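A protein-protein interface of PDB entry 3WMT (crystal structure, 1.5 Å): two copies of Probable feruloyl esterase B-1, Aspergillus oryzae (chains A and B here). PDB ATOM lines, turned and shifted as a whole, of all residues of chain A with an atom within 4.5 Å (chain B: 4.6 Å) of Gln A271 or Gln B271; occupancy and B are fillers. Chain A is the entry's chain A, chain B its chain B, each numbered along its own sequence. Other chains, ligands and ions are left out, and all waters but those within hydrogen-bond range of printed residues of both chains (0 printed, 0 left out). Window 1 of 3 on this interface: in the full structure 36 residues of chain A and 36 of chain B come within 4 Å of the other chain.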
ATOM      1  N   CYS A 253      21.625  17.993 -19.000  1.00  0.00           N
ATOM      2  CA  CYS A 253      21.242  18.007 -20.440  1.00  0.00           C
ATOM      3  C   CYS A 253      20.034  18.771 -20.806  1.00  0.00           C
ATOM      4  O   CYS A 253      19.912  19.124 -22.000  1.00  0.00           O
ATOM      5  CB  CYS A 253      21.102  16.571 -20.885  1.00  0.00           C
ATOM      6  SG  CYS A 253      22.641  15.685 -20.859  1.00  0.00           S
ATOM      7  N   ASP A 268      21.232  13.441 -28.581  1.00  0.00           N
ATOM      8  CA  ASP A 268      22.593  13.297 -29.134  1.00  0.00           C
ATOM      9  C   ASP A 268      23.563  14.279 -28.435  1.00  0.00           C
ATOM     10  O   ASP A 268      24.735  13.952 -28.289  1.00  0.00           O
ATOM     11  CB  ASP A 268      22.597  13.582 -30.622  1.00  0.00           C
ATOM     12  CG  ASP A 268      21.806  12.608 -31.443  1.00  0.00           C
ATOM     13  OD1 ASP A 268      21.520  11.510 -31.001  1.00  0.00           O
ATOM     14  OD2 ASP A 268      21.458  12.970 -32.593  1.00  0.00           O
ATOM     15  N   LEU A 269      23.089  15.428 -28.023  1.00  0.00           N
ATOM     16  CA  LEU A 269      23.974  16.373 -27.353  1.00  0.00           C
ATOM     17  C   LEU A 269      24.290  16.026 -25.935  1.00  0.00           C
ATOM     18  O   LEU A 269      25.224  16.576 -25.333  1.00  0.00           O
ATOM     19  CB  LEU A 269      23.336  17.787 -27.320  1.00  0.00           C
ATOM     20  CG  LEU A 269      23.332  18.590 -28.640  1.00  0.00           C
ATOM     21  CD1 LEU A 269      22.607  17.940 -29.776  1.00  0.00           C
ATOM     22  CD2 LEU A 269      22.764  20.002 -28.318  1.00  0.00           C
ATOM     23  N   CYS A 270      23.522  15.096 -25.382  1.00  0.00           N
ATOM     24  CA  CYS A 270      23.584  14.676 -23.978  1.00  0.00           C
ATOM     25  C   CYS A 270      24.553  13.505 -23.845  1.00  0.00           C
ATOM     26  O   CYS A 270      24.220  12.387 -24.265  1.00  0.00           O
ATOM     27  CB  CYS A 270      22.212  14.335 -23.512  1.00  0.00           C
ATOM     28  SG  CYS A 270      22.158  13.913 -21.724  1.00  0.00           S
ATOM     29  N   GLN A 271      25.672  13.780 -23.238  1.00  0.00           N
ATOM     30  CA  GLN A 271      26.748  12.882 -23.048  1.00  0.00           C
ATOM     31  C   GLN A 271      27.048  12.902 -21.583  1.00  0.00           C
ATOM     32  O   GLN A 271      28.036  13.498 -21.093  1.00  0.00           O
ATOM     33  CB  GLN A 271      27.935  13.162 -23.947  1.00  0.00           C
ATOM     34  CG  GLN A 271      27.636  13.218 -25.442  1.00  0.00           C
ATOM     35  CD  GLN A 271      27.225  11.902 -26.053  1.00  0.00           C
ATOM     36  OE1 GLN A 271      27.770  10.872 -25.616  1.00  0.00           O
ATOM     37  NE2 GLN A 271      26.350  11.853 -27.008  1.00  0.00           N
ATOM     38  N   PRO A 272      26.202  12.252 -20.766  1.00  0.00           N
ATOM     39  CA  PRO A 272      26.190  12.590 -19.331  1.00  0.00           C
ATOM     40  C   PRO A 272      27.384  12.025 -18.591  1.00  0.00           C
ATOM     41  O   PRO A 272      27.948  11.004 -18.961  1.00  0.00           O
ATOM     42  CB  PRO A 272      24.889  11.992 -18.853  1.00  0.00           C
ATOM     43  CG  PRO A 272      24.635  10.857 -19.762  1.00  0.00           C
ATOM     44  CD  PRO A 272      25.099  11.335 -21.107  1.00  0.00           C
ATOM     45  N   ILE A 273      27.817  12.771 -17.587  1.00  0.00           N
ATOM     46  CA  ILE A 273      28.967  12.398 -16.751  1.00  0.00           C
ATOM     47  C   ILE A 273      28.345  11.860 -15.444  1.00  0.00           C
ATOM     48  O   ILE A 273      27.987  12.592 -14.510  1.00  0.00           O
ATOM     49  CB  ILE A 273      29.913  13.545 -16.570  1.00  0.00           C
ATOM     50  CG1 ILE A 273      30.437  14.029 -17.892  1.00  0.00           C
ATOM     51  CG2 ILE A 273      31.041  13.104 -15.610  1.00  0.00           C
ATOM     52  CD1 ILE A 273      31.056  15.360 -17.868  1.00  0.00           C
ATOM     53  N   ARG A 317      23.956   3.095 -28.126  1.00  0.00           N
ATOM     54  CA  ARG A 317      23.633   3.252 -26.764  1.00  0.00           C
ATOM     55  C   ARG A 317      22.124   3.419 -26.565  1.00  0.00           C
ATOM     56  O   ARG A 317      21.384   3.875 -27.486  1.00  0.00           O
ATOM     57  CB  ARG A 317      24.269   4.465 -26.110  1.00  0.00           C
ATOM     58  CG  ARG A 317      23.818   5.813 -26.632  1.00  0.00           C
ATOM     59  CD  ARG A 317      24.420   6.996 -25.923  1.00  0.00           C
ATOM     60  NE  ARG A 317      23.851   8.229 -26.469  1.00  0.00           N
ATOM     61  CZ  ARG A 317      23.996   9.451 -25.929  1.00  0.00           C
ATOM     62  NH1 ARG A 317      24.701   9.652 -24.879  1.00  0.00           N
ATOM     63  NH2 ARG A 317      23.319  10.453 -26.500  1.00  0.00           N
ATOM     64  N   GLN B 252      27.237  23.235 -37.201  1.00  0.00           N
ATOM     65  CA  GLN B 252      26.372  22.442 -36.370  1.00  0.00           C
ATOM     66  C   GLN B 252      26.658  22.578 -34.867  1.00  0.00           C
ATOM     67  O   GLN B 252      25.764  22.404 -34.109  1.00  0.00           O
ATOM     68  CB  GLN B 252      26.508  20.989 -36.752  1.00  0.00           C
ATOM     69  CG  GLN B 252      25.842  20.606 -38.069  1.00  0.00           C
ATOM     70  CD  GLN B 252      25.884  19.139 -38.415  1.00  0.00           C
ATOM     71  OE1 GLN B 252      25.879  18.261 -37.539  1.00  0.00           O
ATOM     72  NE2 GLN B 252      25.878  18.818 -39.722  1.00  0.00           N
ATOM     73  N   CYS B 253      27.909  22.847 -34.538  1.00  0.00           N
ATOM     74  CA  CYS B 253      28.350  22.707 -33.169  1.00  0.00           C
ATOM     75  C   CYS B 253      28.831  23.947 -32.439  1.00  0.00           C
ATOM     76  O   CYS B 253      28.796  23.964 -31.203  1.00  0.00           O
ATOM     77  CB  CYS B 253      29.449  21.638 -33.081  1.00  0.00           C
ATOM     78  SG  CYS B 253      28.784  20.003 -33.539  1.00  0.00           S
ATOM     79  N   ASP B 268      32.086  17.222 -26.587  1.00  0.00           N
ATOM     80  CA  ASP B 268      31.192  16.104 -26.250  1.00  0.00           C
ATOM     81  C   ASP B 268      29.786  16.334 -26.757  1.00  0.00           C
ATOM     82  O   ASP B 268      29.078  15.448 -27.095  1.00  0.00           O
ATOM     83  CB  ASP B 268      31.178  15.878 -24.739  1.00  0.00           C
ATOM     84  CG  ASP B 268      32.543  15.491 -24.166  1.00  0.00           C
ATOM     85  OD1 ASP B 268      33.442  15.029 -24.872  1.00  0.00           O
ATOM     86  OD2 ASP B 268      32.681  15.689 -22.929  1.00  0.00           O
ATOM     87  N   LEU B 269      29.361  17.596 -26.776  1.00  0.00           N
ATOM     88  CA  LEU B 269      28.017  17.938 -27.245  1.00  0.00           C
ATOM     89  C   LEU B 269      27.895  17.838 -28.725  1.00  0.00           C
ATOM     90  O   LEU B 269      26.763  17.812 -29.241  1.00  0.00           O
ATOM     91  CB  LEU B 269      27.684  19.386 -26.864  1.00  0.00           C
ATOM     92  CG  LEU B 269      27.294  19.574 -25.372  1.00  0.00           C
ATOM     93  CD1 LEU B 269      28.250  19.164 -24.302  1.00  0.00           C
ATOM     94  CD2 LEU B 269      26.828  21.073 -25.257  1.00  0.00           C
ATOM     95  N   CYS B 270      29.010  17.802 -29.439  1.00  0.00           N
ATOM     96  CA  CYS B 270      29.075  17.820 -30.926  1.00  0.00           C
ATOM     97  C   CYS B 270      29.092  16.398 -31.463  1.00  0.00           C
ATOM     98  O   CYS B 270      30.090  15.686 -31.297  1.00  0.00           O
ATOM     99  CB  CYS B 270      30.306  18.599 -31.362  1.00  0.00           C
ATOM    100  SG  CYS B 270      30.411  18.808 -33.134  1.00  0.00           S
ATOM    101  N   GLN B 271      28.015  16.032 -32.119  1.00  0.00           N
ATOM    102  CA  GLN B 271      27.793  14.722 -32.672  1.00  0.00           C
ATOM    103  C   GLN B 271      27.417  14.970 -34.086  1.00  0.00           C
ATOM    104  O   GLN B 271      26.206  14.950 -34.478  1.00  0.00           O
ATOM    105  CB  GLN B 271      26.740  13.913 -31.881  1.00  0.00           C
ATOM    106  CG  GLN B 271      27.120  13.751 -30.395  1.00  0.00           C
ATOM    107  CD  GLN B 271      28.356  12.948 -30.083  1.00  0.00           C
ATOM    108  OE1 GLN B 271      28.570  11.965 -30.823  1.00  0.00           O
ATOM    109  NE2 GLN B 271      29.076  13.186 -29.044  1.00  0.00           N
ATOM    110  N   PRO B 272      28.371  15.315 -34.936  1.00  0.00           N
ATOM    111  CA  PRO B 272      28.018  15.917 -36.217  1.00  0.00           C
ATOM    112  C   PRO B 272      27.377  14.939 -37.186  1.00  0.00           C
ATOM    113  O   PRO B 272      27.645  13.744 -37.223  1.00  0.00           O
ATOM    114  CB  PRO B 272      29.358  16.440 -36.703  1.00  0.00           C
ATOM    115  CG  PRO B 272      30.365  15.513 -36.098  1.00  0.00           C
ATOM    116  CD  PRO B 272      29.812  15.180 -34.716  1.00  0.00           C
ATOM    117  N   ILE B 273      26.454  15.505 -37.960  1.00  0.00           N
ATOM    118  CA  ILE B 273      25.766  14.754 -39.035  1.00  0.00           C
ATOM    119  C   ILE B 273      26.370  15.089 -40.389  1.00  0.00           C
ATOM    120  O   ILE B 273      26.109  16.126 -40.987  1.00  0.00           O
ATOM    121  CB  ILE B 273      24.251  15.026 -38.996  1.00  0.00           C
ATOM    122  CG1 ILE B 273      23.675  14.593 -37.658  1.00  0.00           C
ATOM    123  CG2 ILE B 273      23.573  14.287 -40.144  1.00  0.00           C
ATOM    124  CD1 ILE B 273      22.345  15.177 -37.312  1.00  0.00           C
ATOM    125  N   ARG B 317      36.686   8.175 -30.213  1.00  0.00           N
ATOM    126  CA  ARG B 317      36.702   8.914 -31.431  1.00  0.00           C
ATOM    127  C   ARG B 317      37.701  10.063 -31.392  1.00  0.00           C
ATOM    128  O   ARG B 317      38.060  10.592 -30.317  1.00  0.00           O
ATOM    129  CB  ARG B 317      35.291   9.498 -31.781  1.00  0.00           C
ATOM    130  CG  ARG B 317      34.859  10.630 -30.854  1.00  0.00           C
ATOM    131  CD  ARG B 317      33.571  11.303 -31.271  1.00  0.00           C
ATOM    132  NE  ARG B 317      33.284  12.401 -30.330  1.00  0.00           N
ATOM    133  CZ  ARG B 317      32.332  13.311 -30.518  1.00  0.00           C
ATOM    134  NH1 ARG B 317      31.534  13.284 -31.560  1.00  0.00           N
ATOM    135  NH2 ARG B 317      32.317  14.308 -29.629  1.00  0.00           N
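The side-chain amide nitrogen of Gln A271 sits at hydrogen-bond distance from the backbone carbonyl oxygen of Asp A268 (2.9 Å). The side-chain amide nitrogen (NE2) of Gln A271 lies close to the guanidinium group (NH2) of Arg A317, 3.4 Å away. The backbone carbonyl oxygen of Asp B268 sits at hydrogen-bond distance from the side-chain amide nitrogen of Gln B271. The guanidinium group (NH1) of Arg B317 sits at hydrogen-bond distance from the side-chain amide oxygen (OE1) of Gln B271. SG of Cys A270 forms a disulfide with SG of Cys A253, 2.0 Å away. The side-chain sulfur (SG) of Cys B253 forms a disulfide with the side-chain sulfur (SG) of Cys B270 (2.1 Å).
Of the 9 printed residues of chain B, 3 touch a printed residue of chain A. Among the printed residues, 4 pairs touch across the chains.
Gln B271 touches Asp A268. CG of Leu A269 touches O of Leu B269, 3.6 Å away. Gln A271 touches Asp B268 (CG to O, 3.1 Å). NE2 of Gln B271 touches NE2 of Gln A271, at 3.7 Å.
Of the printed residues of chain B, Asp A268 touches Gln B271. Printed residues of chain B within 4 Å of Leu A269: Leu B269. Printed residues of chain B within 4 Å of Gln A271: Asp B268 (3.1 Å) and Gln B271 (3.7 Å). Cys B253 touches none of the printed residues of chain A. Of the printed residues of chain A, Asp B268 touches Gln A271 (3.1 Å). Of the printed residues of chain A, Leu B269 touches Leu A269. Of chain A, only Asp A268 (3.2 Å) and Gln A271 (3.7 Å) come within 4 Å of Gln B271. Arg B317 touches none of the printed residues of chain A. The nearest printed residue of chain B that does not touch Gln A271 is Leu B269 (4.9 Å). The nearest printed residue of chain A that does not touch Gln B271 is Leu A269 (5.0 Å).
Asp A268 touches Gln B271, and with the chains exchanged Gln A271 touches Asp B268. Leu B269 touches its own counterpart, Leu A269. Gln B271 touches its own counterpart, Gln A271. Positions printed for both chains: 253, 268, 269, 270, 271, 272, 273 and 317.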
